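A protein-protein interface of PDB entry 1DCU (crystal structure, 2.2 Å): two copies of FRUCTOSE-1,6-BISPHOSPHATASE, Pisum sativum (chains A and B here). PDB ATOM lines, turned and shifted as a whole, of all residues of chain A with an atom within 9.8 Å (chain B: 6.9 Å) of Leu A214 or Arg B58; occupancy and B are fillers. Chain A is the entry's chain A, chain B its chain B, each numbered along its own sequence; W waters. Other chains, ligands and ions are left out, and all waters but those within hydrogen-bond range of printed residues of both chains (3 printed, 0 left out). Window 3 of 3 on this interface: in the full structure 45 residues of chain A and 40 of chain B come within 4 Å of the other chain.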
ATOM      1  N   TYR A  16      17.114  -9.384   8.181  1.00  0.00           N
ATOM      2  CA  TYR A  16      17.666  -9.378   9.532  1.00  0.00           C
ATOM      3  C   TYR A  16      17.589 -10.784  10.129  1.00  0.00           C
ATOM      4  O   TYR A  16      16.796 -11.652   9.719  1.00  0.00           O
ATOM      5  CB  TYR A  16      16.898  -8.391  10.417  1.00  0.00           C
ATOM      6  CG  TYR A  16      15.426  -8.744  10.541  1.00  0.00           C
ATOM      7  CD1 TYR A  16      15.035  -9.582  11.584  1.00  0.00           C
ATOM      8  CD2 TYR A  16      14.458  -8.295   9.652  1.00  0.00           C
ATOM      9  CE1 TYR A  16      13.702  -9.911  11.729  1.00  0.00           C
ATOM     10  CE2 TYR A  16      13.120  -8.641   9.801  1.00  0.00           C
ATOM     11  CZ  TYR A  16      12.753  -9.464  10.842  1.00  0.00           C
ATOM     12  OH  TYR A  16      11.462  -9.868  11.067  1.00  0.00           O
ATOM     13  N   ILE A  18      16.525 -13.284  13.305  1.00  0.00           N
ATOM     14  CA  ILE A  18      15.714 -13.491  14.463  1.00  0.00           C
ATOM     15  C   ILE A  18      16.117 -14.881  14.991  1.00  0.00           C
ATOM     16  O   ILE A  18      15.927 -15.886  14.313  1.00  0.00           O
ATOM     17  CB  ILE A  18      14.193 -13.405  14.311  1.00  0.00           C
ATOM     18  CG1 ILE A  18      13.592 -14.254  13.191  1.00  0.00           C
ATOM     19  CG2 ILE A  18      13.737 -11.932  14.179  1.00  0.00           C
ATOM     20  CD1 ILE A  18      12.479 -13.585  12.340  1.00  0.00           C
ATOM     21  N   GLN A  57      -0.203 -10.401  33.684  1.00  0.00           N
ATOM     22  CA  GLN A  57      -0.882  -9.540  32.835  1.00  0.00           C
ATOM     23  C   GLN A  57      -2.401  -9.550  33.013  1.00  0.00           C
ATOM     24  O   GLN A  57      -2.888  -8.460  32.806  1.00  0.00           O
ATOM     25  CB  GLN A  57      -0.592  -9.731  31.323  1.00  0.00           C
ATOM     26  CG  GLN A  57       0.822  -9.382  30.905  1.00  0.00           C
ATOM     27  CD  GLN A  57       1.286 -10.068  29.584  1.00  0.00           C
ATOM     28  OE1 GLN A  57       0.533 -10.793  28.969  1.00  0.00           O
ATOM     29  NE2 GLN A  57       2.522  -9.723  29.203  1.00  0.00           N
ATOM     30  N   SER A 193       7.213  -6.659  32.791  1.00  0.00           N
ATOM     31  CA  SER A 193       7.008  -5.215  32.842  1.00  0.00           C
ATOM     32  C   SER A 193       6.478  -4.738  31.503  1.00  0.00           C
ATOM     33  O   SER A 193       5.712  -5.548  30.912  1.00  0.00           O
ATOM     34  CB  SER A 193       8.293  -4.456  33.196  1.00  0.00           C
ATOM     35  OG  SER A 193       9.147  -4.661  32.088  1.00  0.00           O
ATOM     36  N   SER A 194       6.730  -3.527  31.022  1.00  0.00           N
ATOM     37  CA  SER A 194       6.160  -3.140  29.714  1.00  0.00           C
ATOM     38  C   SER A 194       6.614  -4.048  28.588  1.00  0.00           C
ATOM     39  O   SER A 194       5.890  -4.075  27.619  1.00  0.00           O
ATOM     40  CB  SER A 194       6.539  -1.742  29.242  1.00  0.00           C
ATOM     41  OG  SER A 194       7.816  -1.463  29.625  1.00  0.00           O
ATOM     42  N   SER A 195       7.739  -4.754  28.737  1.00  0.00           N
ATOM     43  CA  SER A 195       8.078  -5.870  27.974  1.00  0.00           C
ATOM     44  C   SER A 195       8.425  -7.031  28.922  1.00  0.00           C
ATOM     45  O   SER A 195       8.670  -6.835  30.119  1.00  0.00           O
ATOM     46  CB  SER A 195       9.234  -5.559  26.994  1.00  0.00           C
ATOM     47  OG  SER A 195      10.323  -5.253  27.867  1.00  0.00           O
ATOM     48  N   VAL A 196       8.355  -8.213  28.344  1.00  0.00           N
ATOM     49  CA  VAL A 196       8.695  -9.460  29.021  1.00  0.00           C
ATOM     50  C   VAL A 196      10.103  -9.808  28.535  1.00  0.00           C
ATOM     51  O   VAL A 196      10.344 -10.070  27.359  1.00  0.00           O
ATOM     52  CB  VAL A 196       7.678 -10.577  28.774  1.00  0.00           C
ATOM     53  CG1 VAL A 196       8.090 -11.876  29.550  1.00  0.00           C
ATOM     54  CG2 VAL A 196       6.269 -10.174  29.191  1.00  0.00           C
ATOM     55  N   ILE A 197      11.099  -9.781  29.410  1.00  0.00           N
ATOM     56  CA  ILE A 197      12.523  -9.962  29.142  1.00  0.00           C
ATOM     57  C   ILE A 197      13.079 -11.124  29.996  1.00  0.00           C
ATOM     58  O   ILE A 197      13.126 -11.133  31.251  1.00  0.00           O
ATOM     59  CB  ILE A 197      13.328  -8.702  29.501  1.00  0.00           C
ATOM     60  CG1 ILE A 197      12.773  -7.393  28.834  1.00  0.00           C
ATOM     61  CG2 ILE A 197      14.797  -8.742  29.187  1.00  0.00           C
ATOM     62  CD1 ILE A 197      12.755  -7.484  27.325  1.00  0.00           C
ATOM     63  N   THR A 210      13.742 -11.149  24.335  1.00  0.00           N
ATOM     64  CA  THR A 210      12.507 -10.396  24.440  1.00  0.00           C
ATOM     65  C   THR A 210      11.411 -11.314  23.933  1.00  0.00           C
ATOM     66  O   THR A 210      11.464 -11.829  22.820  1.00  0.00           O
ATOM     67  CB  THR A 210      12.585  -9.071  23.706  1.00  0.00           C
ATOM     68  OG1 THR A 210      13.644  -8.249  24.235  1.00  0.00           O
ATOM     69  CG2 THR A 210      11.305  -8.252  23.892  1.00  0.00           C
ATOM     70  N   LEU A 211      10.370 -11.349  24.762  1.00  0.00           N
ATOM     71  CA  LEU A 211       9.239 -12.177  24.421  1.00  0.00           C
ATOM     72  C   LEU A 211       8.509 -11.406  23.267  1.00  0.00           C
ATOM     73  O   LEU A 211       8.285 -10.194  23.361  1.00  0.00           O
ATOM     74  CB  LEU A 211       8.234 -12.396  25.548  1.00  0.00           C
ATOM     75  CG  LEU A 211       6.935 -13.116  25.221  1.00  0.00           C
ATOM     76  CD1 LEU A 211       7.162 -14.547  24.715  1.00  0.00           C
ATOM     77  CD2 LEU A 211       6.014 -13.130  26.468  1.00  0.00           C
ATOM     78  N   ASP A 212       8.196 -12.131  22.176  1.00  0.00           N
ATOM     79  CA  ASP A 212       7.476 -11.533  21.053  1.00  0.00           C
ATOM     80  C   ASP A 212       6.044 -11.878  21.323  1.00  0.00           C
ATOM     81  O   ASP A 212       5.748 -13.037  21.201  1.00  0.00           O
ATOM     82  CB  ASP A 212       7.834 -12.061  19.642  1.00  0.00           C
ATOM     83  CG  ASP A 212       7.266 -11.163  18.540  1.00  0.00           C
ATOM     84  OD1 ASP A 212       6.184 -10.590  18.763  1.00  0.00           O
ATOM     85  OD2 ASP A 212       7.801 -10.841  17.475  1.00  0.00           O
ATOM     86  N   PRO A 213       5.220 -10.952  21.803  1.00  0.00           N
ATOM     87  CA  PRO A 213       3.815 -11.268  22.090  1.00  0.00           C
ATOM     88  C   PRO A 213       3.029 -11.730  20.860  1.00  0.00           C
ATOM     89  O   PRO A 213       2.115 -12.549  21.064  1.00  0.00           O
ATOM     90  CB  PRO A 213       3.217  -9.985  22.693  1.00  0.00           C
ATOM     91  CG  PRO A 213       4.392  -9.107  22.848  1.00  0.00           C
ATOM     92  CD  PRO A 213       5.493  -9.518  21.894  1.00  0.00           C
ATOM     93  N   LEU A 214       3.489 -11.327  19.632  1.00  0.00           N
ATOM     94  CA  LEU A 214       2.753 -11.863  18.478  1.00  0.00           C
ATOM     95  C   LEU A 214       2.890 -13.330  18.273  1.00  0.00           C
ATOM     96  O   LEU A 214       1.980 -14.064  17.884  1.00  0.00           O
ATOM     97  CB  LEU A 214       3.231 -11.097  17.258  1.00  0.00           C
ATOM     98  CG  LEU A 214       3.069  -9.583  17.436  1.00  0.00           C
ATOM     99  CD1 LEU A 214       3.404  -8.868  16.144  1.00  0.00           C
ATOM    100  CD2 LEU A 214       1.732  -9.172  18.036  1.00  0.00           C
ATOM    101  N   TYR A 215       4.137 -13.783  18.438  1.00  0.00           N
ATOM    102  CA  TYR A 215       4.527 -15.140  18.105  1.00  0.00           C
ATOM    103  C   TYR A 215       4.819 -16.032  19.281  1.00  0.00           C
ATOM    104  O   TYR A 215       4.941 -17.246  19.026  1.00  0.00           O
ATOM    105  CB  TYR A 215       5.652 -15.138  17.046  1.00  0.00           C
ATOM    106  CG  TYR A 215       5.315 -14.098  15.982  1.00  0.00           C
ATOM    107  CD1 TYR A 215       6.127 -12.994  15.778  1.00  0.00           C
ATOM    108  CD2 TYR A 215       4.148 -14.282  15.211  1.00  0.00           C
ATOM    109  CE1 TYR A 215       5.817 -12.059  14.791  1.00  0.00           C
ATOM    110  CE2 TYR A 215       3.815 -13.329  14.260  1.00  0.00           C
ATOM    111  CZ  TYR A 215       4.622 -12.251  14.050  1.00  0.00           C
ATOM    112  OH  TYR A 215       4.286 -11.342  13.113  1.00  0.00           O
ATOM    113  N   GLY A 216       4.804 -15.522  20.510  1.00  0.00           N
ATOM    114  CA  GLY A 216       4.850 -16.486  21.619  1.00  0.00           C
ATOM    115  C   GLY A 216       6.241 -17.075  21.831  1.00  0.00           C
ATOM    116  O   GLY A 216       6.363 -18.179  22.358  1.00  0.00           O
ATOM    117  N   GLU A 217       7.288 -16.439  21.397  1.00  0.00           N
ATOM    118  CA  GLU A 217       8.631 -16.885  21.586  1.00  0.00           C
ATOM    119  C   GLU A 217       9.521 -15.768  22.119  1.00  0.00           C
ATOM    120  O   GLU A 217       9.434 -14.653  21.599  1.00  0.00           O
ATOM    121  CB  GLU A 217       9.291 -17.132  20.165  1.00  0.00           C
ATOM    122  CG  GLU A 217       8.453 -17.990  19.228  1.00  0.00           C
ATOM    123  CD  GLU A 217       8.865 -19.468  19.228  1.00  0.00           C
ATOM    124  OE1 GLU A 217      10.082 -19.780  19.156  1.00  0.00           O
ATOM    125  OE2 GLU A 217       7.915 -20.279  19.233  1.00  0.00           O
ATOM    126  N   PHE A 218      10.588 -16.121  22.806  1.00  0.00           N
ATOM    127  CA  PHE A 218      11.578 -15.159  23.209  1.00  0.00           C
ATOM    128  C   PHE A 218      12.512 -14.991  22.048  1.00  0.00           C
ATOM    129  O   PHE A 218      12.960 -16.035  21.556  1.00  0.00           O
ATOM    130  CB  PHE A 218      12.364 -15.712  24.423  1.00  0.00           C
ATOM    131  CG  PHE A 218      11.536 -15.651  25.702  1.00  0.00           C
ATOM    132  CD1 PHE A 218      11.409 -14.417  26.335  1.00  0.00           C
ATOM    133  CD2 PHE A 218      10.855 -16.752  26.160  1.00  0.00           C
ATOM    134  CE1 PHE A 218      10.654 -14.292  27.482  1.00  0.00           C
ATOM    135  CE2 PHE A 218      10.143 -16.672  27.374  1.00  0.00           C
ATOM    136  CZ  PHE A 218      10.096 -15.449  27.997  1.00  0.00           C
ATOM    137  N   VAL A 219      12.958 -13.809  21.744  1.00  0.00           N
ATOM    138  CA  VAL A 219      13.862 -13.567  20.628  1.00  0.00           C
ATOM    139  C   VAL A 219      15.099 -12.889  21.152  1.00  0.00           C
ATOM    140  O   VAL A 219      15.047 -11.967  21.980  1.00  0.00           O
ATOM    141  CB  VAL A 219      13.096 -12.644  19.564  1.00  0.00           C
ATOM    142  CG1 VAL A 219      14.115 -11.991  18.640  1.00  0.00           C
ATOM    143  CG2 VAL A 219      12.061 -13.493  18.826  1.00  0.00           C
ATOM    144  N   LEU A 220      16.253 -13.363  20.728  1.00  0.00           N
ATOM    145  CA  LEU A 220      17.530 -12.809  21.222  1.00  0.00           C
ATOM    146  C   LEU A 220      17.570 -11.366  20.767  1.00  0.00           C
ATOM    147  O   LEU A 220      17.233 -11.111  19.598  1.00  0.00           O
ATOM    148  CB  LEU A 220      18.651 -13.693  20.648  1.00  0.00           C
ATOM    149  CG  LEU A 220      20.035 -13.053  20.673  1.00  0.00           C
ATOM    150  CD1 LEU A 220      20.554 -12.899  22.114  1.00  0.00           C
ATOM    151  CD2 LEU A 220      21.033 -13.874  19.856  1.00  0.00           C
ATOM    152  N   THR A 221      17.827 -10.401  21.635  1.00  0.00           N
ATOM    153  CA  THR A 221      17.777  -9.020  21.218  1.00  0.00           C
ATOM    154  C   THR A 221      19.029  -8.384  21.780  1.00  0.00           C
ATOM    155  O   THR A 221      19.391  -7.286  21.446  1.00  0.00           O
ATOM    156  CB  THR A 221      16.502  -8.294  21.747  1.00  0.00           C
ATOM    157  OG1 THR A 221      16.440  -8.393  23.167  1.00  0.00           O
ATOM    158  CG2 THR A 221      15.212  -8.824  21.196  1.00  0.00           C
ATOM    159  N   ILE B  52      -0.191   1.124  20.461  1.00  0.00           N
ATOM    160  CA  ILE B  52       1.009   1.621  21.111  1.00  0.00           C
ATOM    161  C   ILE B  52       1.498   0.582  22.122  1.00  0.00           C
ATOM    162  O   ILE B  52       2.719   0.399  22.264  1.00  0.00           O
ATOM    163  CB  ILE B  52       0.781   3.003  21.776  1.00  0.00           C
ATOM    164  CG1 ILE B  52       0.489   4.040  20.672  1.00  0.00           C
ATOM    165  CG2 ILE B  52       1.908   3.451  22.708  1.00  0.00           C
ATOM    166  CD1 ILE B  52       0.012   5.369  21.246  1.00  0.00           C
ATOM    167  N   ALA B  53       0.579  -0.040  22.900  1.00  0.00           N
ATOM    168  CA  ALA B  53       1.076  -1.072  23.824  1.00  0.00           C
ATOM    169  C   ALA B  53       1.994  -2.101  23.174  1.00  0.00           C
ATOM    170  O   ALA B  53       3.075  -2.432  23.645  1.00  0.00           O
ATOM    171  CB  ALA B  53      -0.070  -1.794  24.506  1.00  0.00           C
ATOM    172  N   SER B  54       1.595  -2.706  22.084  1.00  0.00           N
ATOM    173  CA  SER B  54       2.270  -3.635  21.224  1.00  0.00           C
ATOM    174  C   SER B  54       3.561  -3.023  20.705  1.00  0.00           C
ATOM    175  O   SER B  54       4.600  -3.725  20.931  1.00  0.00           O
ATOM    176  CB  SER B  54       1.244  -3.895  20.063  1.00  0.00           C
ATOM    177  OG  SER B  54       1.801  -5.024  19.433  1.00  0.00           O
ATOM    178  N   LEU B  55       3.617  -1.749  20.338  1.00  0.00           N
ATOM    179  CA  LEU B  55       4.894  -1.176  19.940  1.00  0.00           C
ATOM    180  C   LEU B  55       5.880  -1.196  21.099  1.00  0.00           C
ATOM    181  O   LEU B  55       7.051  -1.402  20.956  1.00  0.00           O
ATOM    182  CB  LEU B  55       4.733   0.305  19.540  1.00  0.00           C
ATOM    183  CG  LEU B  55       3.959   0.485  18.223  1.00  0.00           C
ATOM    184  CD1 LEU B  55       3.844   2.014  17.939  1.00  0.00           C
ATOM    185  CD2 LEU B  55       4.665  -0.190  17.017  1.00  0.00           C
ATOM    186  N   VAL B  56       5.472  -0.748  22.285  1.00  0.00           N
ATOM    187  CA  VAL B  56       6.219  -0.650  23.500  1.00  0.00           C
ATOM    188  C   VAL B  56       6.682  -2.075  23.849  1.00  0.00           C
ATOM    189  O   VAL B  56       7.867  -2.316  24.093  1.00  0.00           O
ATOM    190  CB  VAL B  56       5.377   0.015  24.625  1.00  0.00           C
ATOM    191  CG1 VAL B  56       6.005  -0.323  25.968  1.00  0.00           C
ATOM    192  CG2 VAL B  56       5.353   1.580  24.426  1.00  0.00           C
ATOM    193  N   GLN B  57       5.870  -3.095  23.717  1.00  0.00           N
ATOM    194  CA  GLN B  57       6.248  -4.425  24.137  1.00  0.00           C
ATOM    195  C   GLN B  57       7.310  -5.044  23.222  1.00  0.00           C
ATOM    196  O   GLN B  57       8.088  -5.860  23.692  1.00  0.00           O
ATOM    197  CB  GLN B  57       5.074  -5.411  24.103  1.00  0.00           C
ATOM    198  CG  GLN B  57       4.098  -5.204  25.227  1.00  0.00           C
ATOM    199  CD  GLN B  57       2.724  -5.794  25.027  1.00  0.00           C
ATOM    200  OE1 GLN B  57       2.331  -6.427  24.048  1.00  0.00           O
ATOM    201  NE2 GLN B  57       1.934  -5.480  26.071  1.00  0.00           N
ATOM    202  N   ARG B  58       7.274  -4.702  21.940  1.00  0.00           N
ATOM    203  CA  ARG B  58       8.104  -5.364  20.938  1.00  0.00           C
ATOM    204  C   ARG B  58       9.256  -4.455  20.559  1.00  0.00           C
ATOM    205  O   ARG B  58       9.907  -4.800  19.604  1.00  0.00           O
ATOM    206  CB  ARG B  58       7.291  -5.586  19.621  1.00  0.00           C
ATOM    207  CG  ARG B  58       6.279  -6.704  19.800  1.00  0.00           C
ATOM    208  CD  ARG B  58       5.574  -7.183  18.548  1.00  0.00           C
ATOM    209  NE  ARG B  58       6.416  -8.148  17.785  1.00  0.00           N
ATOM    210  CZ  ARG B  58       6.964  -7.651  16.646  1.00  0.00           C
ATOM    211  NH1 ARG B  58       6.800  -6.386  16.253  1.00  0.00           N
ATOM    212  NH2 ARG B  58       7.695  -8.449  15.873  1.00  0.00           N
ATOM    213  N   ALA B  59       9.325  -3.295  21.175  1.00  0.00           N
ATOM    214  CA  ALA B  59      10.402  -2.383  20.826  1.00  0.00           C
ATOM    215  C   ALA B  59      11.767  -3.058  20.736  1.00  0.00           C
ATOM    216  O   ALA B  59      12.531  -2.564  19.875  1.00  0.00           O
ATOM    217  CB  ALA B  59      10.481  -1.173  21.750  1.00  0.00           C
ATOM    218  N   ASN B  60      12.206  -3.976  21.554  1.00  0.00           N
ATOM    219  CA  ASN B  60      13.596  -4.488  21.401  1.00  0.00           C
ATOM    220  C   ASN B  60      13.736  -5.245  20.102  1.00  0.00           C
ATOM    221  O   ASN B  60      14.773  -5.307  19.477  1.00  0.00           O
ATOM    222  CB  ASN B  60      13.937  -5.450  22.582  1.00  0.00           C
ATOM    223  CG  ASN B  60      14.119  -4.650  23.877  1.00  0.00           C
ATOM    224  OD1 ASN B  60      14.339  -3.446  23.861  1.00  0.00           O
ATOM    225  ND2 ASN B  60      14.026  -5.274  25.035  1.00  0.00           N
ATOM    226  N   ILE B  61      12.683  -5.965  19.723  1.00  0.00           N
ATOM    227  CA  ILE B  61      12.580  -6.773  18.551  1.00  0.00           C
ATOM    228  C   ILE B  61      12.533  -5.912  17.289  1.00  0.00           C
ATOM    229  O   ILE B  61      13.347  -6.082  16.386  1.00  0.00           O
ATOM    230  CB  ILE B  61      11.369  -7.654  18.669  1.00  0.00           C
ATOM    231  CG1 ILE B  61      11.611  -8.548  19.928  1.00  0.00           C
ATOM    232  CG2 ILE B  61      11.085  -8.442  17.390  1.00  0.00           C
ATOM    233  CD1 ILE B  61      10.379  -9.376  20.252  1.00  0.00           C
ATOM    234  N   SER B  62      11.708  -4.865  17.276  1.00  0.00           N
ATOM    235  CA  SER B  62      11.489  -3.874  16.254  1.00  0.00           C
ATOM    236  C   SER B  62      12.791  -3.119  15.942  1.00  0.00           C
ATOM    237  O   SER B  62      13.135  -3.063  14.777  1.00  0.00           O
ATOM    238  CB  SER B  62      10.356  -2.858  16.541  1.00  0.00           C
ATOM    239  N   ASN B  63      13.589  -2.733  16.920  1.00  0.00           N
ATOM    240  CA  ASN B  63      14.874  -2.089  16.725  1.00  0.00           C
ATOM    241  C   ASN B  63      16.017  -2.949  16.177  1.00  0.00           C
ATOM    242  O   ASN B  63      17.037  -2.415  15.693  1.00  0.00           O
ATOM    243  CB  ASN B  63      15.243  -1.362  18.032  1.00  0.00           C
ATOM    244  CG  ASN B  63      14.479  -0.054  18.214  1.00  0.00           C
ATOM    245  OD1 ASN B  63      14.258   0.693  17.247  1.00  0.00           O
ATOM    246  ND2 ASN B  63      14.023   0.297  19.413  1.00  0.00           N
HETATM  247  O   HOH W   1      13.199  -3.968  27.757  1.00  0.00           O
HETATM  248  O   HOH W   2       2.995  -3.579  28.013  1.00  0.00           O
HETATM  249  O   HOH W   3       7.993  -8.158  25.343  1.00  0.00           O
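1 position is printed for both chains. Of the 14 pairs that touch across the chains among the printed residues, none has its exchanged pair printed and touching as well.
Water W3 lies within hydrogen-bond range of O of Gln B57 (2.8 Å), O of Leu A211 (2.9 Å) and N of Val A196 (3.0 Å). Water W2 lies within hydrogen-bond range of NE2 of Gln B57 (2.9 Å) and O of Ser A194 (3.0 Å). Water W1 bridges the side-chain amide nitrogen (ND2) of Asn B60 (3.1 Å) and the side-chain hydroxyl (OG) of Ser A195 (3.2 Å).
Among the printed residues, merely in contact across the chains: Ser A194 with Val B56 (3.6 Å), Ser A194 with Gln B57 (3.2 Å), Ser A195 with Gln B57 (3.5 Å), Ile A197 with Asn B60 (3.4 Å), Thr A210 with Ile B61 (3.7 Å), Leu A211 with Ile B61 (3.8 Å), Asp A212 with Ile B61 (3.7 Å), Pro A213 with Gln B57 (3.6 Å), Pro A213 with Arg B58 (3.6 Å), Leu A214 with Arg B58 (3.5 Å), Thr A221 with Asn B60 (3.9 Å) and Thr A221 with Ile B61 (3.8 Å).
Hydrophobic or aromatic side chains of chain B within 4 Å of the printed part of chain A: Val B56 and Ile B61. Of the 20 printed residues of chain A, 9 touch a printed residue of chain B. Hydrophobic or aromatic side chains of chain A that line the printed part of chain B: Ile A197, Pro A213 and Leu A214. Among the printed residues, 14 pairs touch across the chains. Among the printed residues, Asp or Glu carboxylates within 4 Å of a Lys or Arg side-chain nitrogen of the other chain: Asp A212 with Arg B58 (2.6 Å).
The side-chain hydroxyl of Ser A193 sits at hydrogen-bond distance from the backbone carbonyl oxygen of Ser A195 (3.0 Å). O of Val A196 sits at hydrogen-bond distance from N of Leu A211, 2.9 Å away. The backbone NH (N) of Val A219 lies within hydrogen-bond range of the backbone carbonyl oxygen (O) of Thr A210, at 2.7 Å. OG1 of Thr A210 is in hydrogen-bond range of OG1 of Thr A221. The backbone NH (N) of Leu A214 sits at hydrogen-bond distance from the side-chain carboxylate (OD1) of Asp A212, at 2.9 Å. The backbone NH (N) of Asp A212 is in hydrogen-bond range of the backbone carbonyl oxygen (O) of Glu A217.
The side-chain amide nitrogen (ND2) of Asn B60 is in hydrogen-bond range of the side-chain hydroxyl (OG1) of Thr A210, 3.1 Å away. The side-chain carboxylate of Asp A212 lies within salt-bridge range of the guanidinium group of Arg B58, at 2.6 Å.
Tyr A16 touches none of the printed residues of chain B. Of the printed residues of chain B, Thr A210 touches Asn B60 (3.1 Å) and Ile B61 (3.7 Å). Of the printed residues of chain B, Leu A211 touches Ile B61. Tyr A215 touches none of the printed residues of chain B. Of the printed residues of chain A, Val B56 touches Ser A194 (3.6 Å). Of the printed residues of chain A, Gln B57 touches Ser A194 (3.2 Å), Ser A195 (3.5 Å) and Pro A213 (3.6 Å). Arg B58 touches just these residues of chain A: Asp A212 (2.6 Å), Pro A213 (3.6 Å) and Leu A214 (3.5 Å). No residue of chain A comes within 4 Å of Ala B59. Of chain A, only Thr A210 (3.7 Å), Leu A211 (3.8 Å), Asp A212 (3.7 Å) and Thr A221 (3.8 Å) come within 4 Å of Ile B61. The nearest residue of chain B that does not touch Leu A214 is Ser B54 (4.4 Å). The nearest residue of chain A that does not touch Arg B58 is Tyr A215 (4.2 Å).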
